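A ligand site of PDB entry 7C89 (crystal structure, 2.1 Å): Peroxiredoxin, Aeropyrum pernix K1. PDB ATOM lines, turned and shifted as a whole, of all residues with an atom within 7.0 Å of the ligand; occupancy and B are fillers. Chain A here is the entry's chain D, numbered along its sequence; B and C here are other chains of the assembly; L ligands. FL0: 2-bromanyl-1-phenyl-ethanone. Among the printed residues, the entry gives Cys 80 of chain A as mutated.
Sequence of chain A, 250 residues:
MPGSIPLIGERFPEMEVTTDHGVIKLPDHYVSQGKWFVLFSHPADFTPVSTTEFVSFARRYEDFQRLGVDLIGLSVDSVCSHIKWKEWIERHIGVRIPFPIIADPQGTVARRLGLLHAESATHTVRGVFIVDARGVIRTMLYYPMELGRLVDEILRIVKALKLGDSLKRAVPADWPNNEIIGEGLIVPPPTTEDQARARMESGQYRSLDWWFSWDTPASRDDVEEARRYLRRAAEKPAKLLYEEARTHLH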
ATOM      1  N   ASP A  77      -5.299  24.469 -14.397  1.00  0.00           N
ATOM      2  CA  ASP A  77      -4.407  23.423 -14.966  1.00  0.00           C
ATOM      3  C   ASP A  77      -3.684  22.660 -13.858  1.00  0.00           C
ATOM      4  O   ASP A  77      -3.593  23.149 -12.710  1.00  0.00           O
ATOM      5  CB  ASP A  77      -3.343  23.979 -15.892  1.00  0.00           C
ATOM      6  CG  ASP A  77      -3.872  24.866 -17.000  1.00  0.00           C
ATOM      7  OD1 ASP A  77      -4.611  24.333 -17.892  1.00  0.00           O
ATOM      8  OD2 ASP A  77      -3.575  26.112 -16.917  1.00  0.00           O
ATOM      9  N   SER A  78      -3.143  21.498 -14.217  1.00  0.00           N
ATOM     10  CA  SER A  78      -2.402  20.601 -13.301  1.00  0.00           C
ATOM     11  C   SER A  78      -0.935  21.037 -13.165  1.00  0.00           C
ATOM     12  O   SER A  78      -0.446  21.827 -13.965  1.00  0.00           O
ATOM     13  CB  SER A  78      -2.543  19.159 -13.740  1.00  0.00           C
ATOM     14  OG  SER A  78      -3.908  18.773 -13.547  1.00  0.00           O
ATOM     15  N   VAL A  79      -0.279  20.514 -12.148  1.00  0.00           N
ATOM     16  CA  VAL A  79       1.166  20.713 -11.877  1.00  0.00           C
ATOM     17  C   VAL A  79       1.984  20.372 -13.131  1.00  0.00           C
ATOM     18  O   VAL A  79       2.930  21.137 -13.451  1.00  0.00           O
ATOM     19  CB  VAL A  79       1.597  19.884 -10.653  1.00  0.00           C
ATOM     20  CG1 VAL A  79       3.108  19.814 -10.530  1.00  0.00           C
ATOM     21  CG2 VAL A  79       0.979  20.432  -9.378  1.00  0.00           C
ATOM     22  N   CYS A  80       1.684  19.244 -13.789  1.00  0.00           N
ATOM     23  CA  CYS A  80       2.517  18.735 -14.918  1.00  0.00           C
ATOM     24  C   CYS A  80       2.474  19.793 -16.034  1.00  0.00           C
ATOM     25  O   CYS A  80       3.530  20.129 -16.655  1.00  0.00           O
ATOM     26  CB  CYS A  80       2.024  17.347 -15.371  1.00  0.00           C
ATOM     27  SG  CYS A  80       2.644  16.061 -14.268  1.00  0.00           S
ATOM     28  N   SER A  81       1.294  20.342 -16.261  1.00  0.00           N
ATOM     29  CA  SER A  81       1.086  21.389 -17.293  1.00  0.00           C
ATOM     30  C   SER A  81       1.856  22.643 -16.860  1.00  0.00           C
ATOM     31  O   SER A  81       2.535  23.237 -17.722  1.00  0.00           O
ATOM     32  CB  SER A  81      -0.405  21.594 -17.513  1.00  0.00           C
ATOM     33  OG  SER A  81      -0.651  22.759 -18.282  1.00  0.00           O
ATOM     34  N   HIS A  82       1.809  23.010 -15.582  1.00  0.00           N
ATOM     35  CA  HIS A  82       2.547  24.197 -15.066  1.00  0.00           C
ATOM     36  C   HIS A  82       4.021  24.043 -15.393  1.00  0.00           C
ATOM     37  O   HIS A  82       4.620  24.984 -15.965  1.00  0.00           O
ATOM     38  CB  HIS A  82       2.373  24.389 -13.551  1.00  0.00           C
ATOM     39  CG  HIS A  82       1.026  24.857 -13.104  1.00  0.00           C
ATOM     40  ND1 HIS A  82       0.059  25.327 -13.979  1.00  0.00           N
ATOM     41  CD2 HIS A  82       0.468  24.879 -11.874  1.00  0.00           C
ATOM     42  CE1 HIS A  82      -1.018  25.647 -13.295  1.00  0.00           C
ATOM     43  NE2 HIS A  82      -0.803  25.367 -12.009  1.00  0.00           N
ATOM     44  N   ILE A  83       4.592  22.881 -15.038  1.00  0.00           N
ATOM     45  CA  ILE A  83       6.031  22.629 -15.237  1.00  0.00           C
ATOM     46  C   ILE A  83       6.348  22.683 -16.738  1.00  0.00           C
ATOM     47  O   ILE A  83       7.321  23.359 -17.077  1.00  0.00           O
ATOM     48  CB  ILE A  83       6.490  21.328 -14.570  1.00  0.00           C
ATOM     49  CG1 ILE A  83       6.240  21.409 -13.056  1.00  0.00           C
ATOM     50  CG2 ILE A  83       7.956  21.048 -14.935  1.00  0.00           C
ATOM     51  CD1 ILE A  83       6.452  20.139 -12.287  1.00  0.00           C
ATOM     52  N   ALA A 103      -2.158  24.642  -8.785  1.00  0.00           N
ATOM     53  CA  ALA A 103      -2.958  23.807  -9.680  1.00  0.00           C
ATOM     54  C   ALA A 103      -4.318  23.658  -9.018  1.00  0.00           C
ATOM     55  O   ALA A 103      -4.368  23.254  -7.858  1.00  0.00           O
ATOM     56  CB  ALA A 103      -2.283  22.466  -9.865  1.00  0.00           C
ATOM     57  N   PRO B  43      -6.257  10.729 -15.624  1.00  0.00           N
ATOM     58  CA  PRO B  43      -6.052  11.753 -14.592  1.00  0.00           C
ATOM     59  C   PRO B  43      -5.566  13.101 -15.140  1.00  0.00           C
ATOM     60  O   PRO B  43      -6.134  14.085 -14.758  1.00  0.00           O
ATOM     61  CB  PRO B  43      -5.001  11.116 -13.646  1.00  0.00           C
ATOM     62  CG  PRO B  43      -4.358   9.996 -14.473  1.00  0.00           C
ATOM     63  CD  PRO B  43      -5.497   9.493 -15.329  1.00  0.00           C
ATOM     64  N   ALA B  44      -4.529  13.139 -15.968  1.00  0.00           N
ATOM     65  CA  ALA B  44      -3.944  14.413 -16.453  1.00  0.00           C
ATOM     66  C   ALA B  44      -3.065  14.153 -17.654  1.00  0.00           C
ATOM     67  O   ALA B  44      -2.503  13.067 -17.770  1.00  0.00           O
ATOM     68  CB  ALA B  44      -3.153  15.110 -15.374  1.00  0.00           C
ATOM     69  N   ASP B  45      -2.934  15.182 -18.478  1.00  0.00           N
ATOM     70  CA  ASP B  45      -2.017  15.251 -19.630  1.00  0.00           C
ATOM     71  C   ASP B  45      -0.586  15.217 -19.081  1.00  0.00           C
ATOM     72  O   ASP B  45      -0.361  15.554 -17.889  1.00  0.00           O
ATOM     73  CB  ASP B  45      -2.330  16.484 -20.473  1.00  0.00           C
ATOM     74  CG  ASP B  45      -3.727  16.517 -21.098  1.00  0.00           C
ATOM     75  OD1 ASP B  45      -4.521  15.517 -20.944  1.00  0.00           O
ATOM     76  OD2 ASP B  45      -4.001  17.515 -21.795  1.00  0.00           O
ATOM     77  N   PHE B  46       0.358  14.750 -19.895  1.00  0.00           N
ATOM     78  CA  PHE B  46       1.774  14.650 -19.483  1.00  0.00           C
ATOM     79  C   PHE B  46       1.879  13.817 -18.214  1.00  0.00           C
ATOM     80  O   PHE B  46       2.664  14.190 -17.297  1.00  0.00           O
ATOM     81  CB  PHE B  46       2.364  16.043 -19.281  1.00  0.00           C
ATOM     82  CG  PHE B  46       2.409  16.886 -20.520  1.00  0.00           C
ATOM     83  CD1 PHE B  46       3.409  16.711 -21.450  1.00  0.00           C
ATOM     84  CD2 PHE B  46       1.464  17.885 -20.739  1.00  0.00           C
ATOM     85  CE1 PHE B  46       3.442  17.463 -22.610  1.00  0.00           C
ATOM     86  CE2 PHE B  46       1.525  18.661 -21.892  1.00  0.00           C
ATOM     87  CZ  PHE B  46       2.497  18.444 -22.828  1.00  0.00           C
ATOM     88  N   THR B  47       1.117  12.720 -18.163  1.00  0.00           N
ATOM     89  CA  THR B  47       1.345  11.611 -17.231  1.00  0.00           C
ATOM     90  C   THR B  47       1.669  10.335 -18.034  1.00  0.00           C
ATOM     91  O   THR B  47       1.211  10.110 -19.180  1.00  0.00           O
ATOM     92  CB  THR B  47       0.205  11.457 -16.220  1.00  0.00           C
ATOM     93  OG1 THR B  47      -0.986  11.134 -16.940  1.00  0.00           O
ATOM     94  CG2 THR B  47       0.025  12.687 -15.361  1.00  0.00           C
ATOM     95  N   PRO B  48       2.566   9.509 -17.464  1.00  0.00           N
ATOM     96  CA  PRO B  48       3.116   8.366 -18.173  1.00  0.00           C
ATOM     97  C   PRO B  48       2.125   7.213 -18.437  1.00  0.00           C
ATOM     98  O   PRO B  48       2.033   6.829 -19.581  1.00  0.00           O
ATOM     99  CB  PRO B  48       4.336   7.995 -17.306  1.00  0.00           C
ATOM    100  CG  PRO B  48       3.965   8.464 -15.908  1.00  0.00           C
ATOM    101  CD  PRO B  48       3.143   9.713 -16.123  1.00  0.00           C
ATOM    102  N   ASP B  77      -7.773  18.683 -17.646  1.00  0.00           N
ATOM    103  CA  ASP B  77      -6.881  19.639 -18.330  1.00  0.00           C
ATOM    104  C   ASP B  77      -7.655  20.421 -19.415  1.00  0.00           C
ATOM    105  O   ASP B  77      -8.657  19.953 -19.917  1.00  0.00           O
ATOM    106  CB  ASP B  77      -5.711  18.935 -19.036  1.00  0.00           C
ATOM    107  CG  ASP B  77      -4.910  17.994 -18.154  1.00  0.00           C
ATOM    108  OD1 ASP B  77      -4.027  18.480 -17.398  1.00  0.00           O
ATOM    109  OD2 ASP B  77      -5.166  16.770 -18.252  1.00  0.00           O
ATOM    110  N   SER B 120      -8.318  10.213  -5.824  1.00  0.00           N
ATOM    111  CA  SER B 120      -7.976  11.645  -6.033  1.00  0.00           C
ATOM    112  C   SER B 120      -9.250  12.503  -6.061  1.00  0.00           C
ATOM    113  O   SER B 120     -10.190  12.169  -6.800  1.00  0.00           O
ATOM    114  CB  SER B 120      -7.153  11.808  -7.286  1.00  0.00           C
ATOM    115  OG  SER B 120      -7.106  13.151  -7.683  1.00  0.00           O
ATOM    116  N   THR B 122      -9.156  15.504  -7.248  1.00  0.00           N
ATOM    117  CA  THR B 122      -8.921  16.517  -8.306  1.00  0.00           C
ATOM    118  C   THR B 122      -8.802  15.895  -9.705  1.00  0.00           C
ATOM    119  O   THR B 122      -9.072  16.635 -10.662  1.00  0.00           O
ATOM    120  CB  THR B 122      -7.679  17.334  -7.987  1.00  0.00           C
ATOM    121  OG1 THR B 122      -6.641  16.371  -7.836  1.00  0.00           O
ATOM    122  CG2 THR B 122      -7.860  18.205  -6.765  1.00  0.00           C
ATOM    123  N   HIS B 123      -8.357  14.641  -9.805  1.00  0.00           N
ATOM    124  CA  HIS B 123      -8.093  13.984 -11.099  1.00  0.00           C
ATOM    125  C   HIS B 123      -8.919  12.708 -11.213  1.00  0.00           C
ATOM    126  O   HIS B 123      -9.065  11.927 -10.279  1.00  0.00           O
ATOM    127  CB  HIS B 123      -6.608  13.777 -11.320  1.00  0.00           C
ATOM    128  CG  HIS B 123      -5.839  15.051 -11.338  1.00  0.00           C
ATOM    129  ND1 HIS B 123      -5.269  15.578 -10.200  1.00  0.00           N
ATOM    130  CD2 HIS B 123      -5.551  15.902 -12.341  1.00  0.00           C
ATOM    131  CE1 HIS B 123      -4.665  16.701 -10.505  1.00  0.00           C
ATOM    132  NE2 HIS B 123      -4.800  16.899 -11.800  1.00  0.00           N
ATOM    133  N   MET B 145      -5.620   4.804 -10.906  1.00  0.00           N
ATOM    134  CA  MET B 145      -4.449   5.620 -11.380  1.00  0.00           C
ATOM    135  C   MET B 145      -3.262   4.709 -11.716  1.00  0.00           C
ATOM    136  O   MET B 145      -2.564   4.991 -12.689  1.00  0.00           O
ATOM    137  CB  MET B 145      -3.950   6.613 -10.327  1.00  0.00           C
ATOM    138  CG  MET B 145      -5.007   7.540  -9.778  1.00  0.00           C
ATOM    139  SD  MET B 145      -5.687   8.503 -11.103  1.00  0.00           S
ATOM    140  CE  MET B 145      -6.537   9.739 -10.129  1.00  0.00           C
ATOM    141  N   PRO C 189       5.435   9.994 -11.486  1.00  0.00           N
ATOM    142  CA  PRO C 189       6.134  11.191 -11.942  1.00  0.00           C
ATOM    143  C   PRO C 189       6.448  12.178 -10.815  1.00  0.00           C
ATOM    144  O   PRO C 189       5.831  12.136  -9.760  1.00  0.00           O
ATOM    145  CB  PRO C 189       5.117  11.821 -12.900  1.00  0.00           C
ATOM    146  CG  PRO C 189       3.792  11.366 -12.348  1.00  0.00           C
ATOM    147  CD  PRO C 189       4.036   9.933 -11.946  1.00  0.00           C
ATOM    148  N   PRO C 190       7.440  13.075 -10.974  1.00  0.00           N
ATOM    149  CA  PRO C 190       7.695  14.114  -9.969  1.00  0.00           C
ATOM    150  C   PRO C 190       6.450  14.975  -9.732  1.00  0.00           C
ATOM    151  O   PRO C 190       5.637  15.078 -10.633  1.00  0.00           O
ATOM    152  CB  PRO C 190       8.802  14.967 -10.594  1.00  0.00           C
ATOM    153  CG  PRO C 190       9.417  14.077 -11.686  1.00  0.00           C
ATOM    154  CD  PRO C 190       8.296  13.193 -12.156  1.00  0.00           C
ATOM    155  N   THR C 191       6.307  15.542  -8.536  1.00  0.00           N
ATOM    156  CA  THR C 191       5.209  16.456  -8.116  1.00  0.00           C
ATOM    157  C   THR C 191       5.748  17.892  -7.943  1.00  0.00           C
ATOM    158  O   THR C 191       4.946  18.766  -7.658  1.00  0.00           O
ATOM    159  CB  THR C 191       4.537  15.930  -6.848  1.00  0.00           C
ATOM    160  OG1 THR C 191       5.489  16.023  -5.779  1.00  0.00           O
ATOM    161  CG2 THR C 191       4.074  14.504  -6.982  1.00  0.00           C
ATOM    162  N   THR C 192       7.048  18.135  -8.113  1.00  0.00           N
ATOM    163  CA  THR C 192       7.649  19.484  -7.949  1.00  0.00           C
ATOM    164  C   THR C 192       8.722  19.674  -9.003  1.00  0.00           C
ATOM    165  O   THR C 192       9.269  18.656  -9.490  1.00  0.00           O
ATOM    166  CB  THR C 192       8.181  19.707  -6.527  1.00  0.00           C
ATOM    167  OG1 THR C 192       9.408  19.001  -6.368  1.00  0.00           O
ATOM    168  CG2 THR C 192       7.188  19.280  -5.467  1.00  0.00           C
ATOM    169  N   TRP C 210      10.863  14.196 -17.992  1.00  0.00           N
ATOM    170  CA  TRP C 210      10.981  14.236 -16.515  1.00  0.00           C
ATOM    171  C   TRP C 210       9.745  13.583 -15.910  1.00  0.00           C
ATOM    172  O   TRP C 210       9.819  13.110 -14.750  1.00  0.00           O
ATOM    173  CB  TRP C 210      11.199  15.662 -15.998  1.00  0.00           C
ATOM    174  CG  TRP C 210      10.112  16.605 -16.357  1.00  0.00           C
ATOM    175  CD1 TRP C 210      10.083  17.485 -17.397  1.00  0.00           C
ATOM    176  CD2 TRP C 210       8.842  16.714 -15.678  1.00  0.00           C
ATOM    177  NE1 TRP C 210       8.895  18.155 -17.394  1.00  0.00           N
ATOM    178  CE2 TRP C 210       8.122  17.704 -16.353  1.00  0.00           C
ATOM    179  CE3 TRP C 210       8.280  16.068 -14.576  1.00  0.00           C
ATOM    180  CZ2 TRP C 210       6.822  18.050 -15.977  1.00  0.00           C
ATOM    181  CZ3 TRP C 210       7.011  16.427 -14.185  1.00  0.00           C
ATOM    182  CH2 TRP C 210       6.307  17.424 -14.860  1.00  0.00           C
ATOM    183  N   TRP C 211       8.647  13.514 -16.656  1.00  0.00           N
ATOM    184  CA  TRP C 211       7.374  12.953 -16.120  1.00  0.00           C
ATOM    185  C   TRP C 211       7.198  11.468 -16.529  1.00  0.00           C
ATOM    186  O   TRP C 211       6.207  10.817 -16.101  1.00  0.00           O
ATOM    187  CB  TRP C 211       6.195  13.835 -16.564  1.00  0.00           C
ATOM    188  CG  TRP C 211       6.163  14.116 -18.038  1.00  0.00           C
ATOM    189  CD1 TRP C 211       6.690  15.162 -18.717  1.00  0.00           C
ATOM    190  CD2 TRP C 211       5.478  13.325 -19.022  1.00  0.00           C
ATOM    191  NE1 TRP C 211       6.392  15.100 -20.047  1.00  0.00           N
ATOM    192  CE2 TRP C 211       5.715  13.929 -20.283  1.00  0.00           C
ATOM    193  CE3 TRP C 211       4.741  12.142 -18.962  1.00  0.00           C
ATOM    194  CZ2 TRP C 211       5.176  13.423 -21.456  1.00  0.00           C
ATOM    195  CZ3 TRP C 211       4.224  11.629 -20.141  1.00  0.00           C
ATOM    196  CH2 TRP C 211       4.413  12.278 -21.359  1.00  0.00           C
HETATM  197  C1  FL0 L   1       2.217  16.292 -12.567  1.00  0.00           C
HETATM  198  C2  FL0 L   1       0.718  16.251 -12.515  1.00  0.00           C
HETATM  199  C3  FL0 L   1      -0.003  14.987 -12.160  1.00  0.00           C
HETATM  200  C4  FL0 L   1       0.694  13.831 -11.806  1.00  0.00           C
HETATM  201  C5  FL0 L   1      -0.027  12.687 -11.463  1.00  0.00           C
HETATM  202  C6  FL0 L   1      -1.416  12.685 -11.494  1.00  0.00           C
HETATM  203  C7  FL0 L   1      -2.101  13.857 -11.856  1.00  0.00           C
HETATM  204  C8  FL0 L   1      -1.399  14.989 -12.206  1.00  0.00           C
HETATM  205  O9  FL0 L   1       0.093  17.267 -12.759  1.00  0.00           O
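Residues that only touch the ligand: Ser 78 (3.4 Å), Ala 44 of chain B (3.6 Å), Thr 47 of chain B (3.8 Å), His 123 of chain B (3.9 Å) and Pro 189 of chain C (3.996 Å). Hydrophobic or aromatic side chains that line the ligand: Val 79, Ala 44 of chain B, His 123 of chain B and Pro 189 of chain C.
A ring nitrogen (NE2) of His 123 of chain B sits at hydrogen-bond distance from the side-chain hydroxyl (OG) of Ser 78 (2.7 Å). O of Ala 44 of chain B is in hydrogen-bond range of OG1 of Thr 47 of chain B, 2.6 Å away. OG of Ser 120 of chain B is in hydrogen-bond range of N of His 123 of chain B (2.9 Å). A ring nitrogen (ND1) of His 123 of chain B lies within hydrogen-bond range of the side-chain hydroxyl of Thr 122 of chain B.
N of Cys 80 sits at hydrogen-bond distance from O9 of the ligand. The side-chain sulfur (SG) of Cys 80 is covalently linked to a carbon (C1) of the ligand, 1.8 Å away. O9 of the ligand is in hydrogen-bond range of N of Val 79 (3.3 Å).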
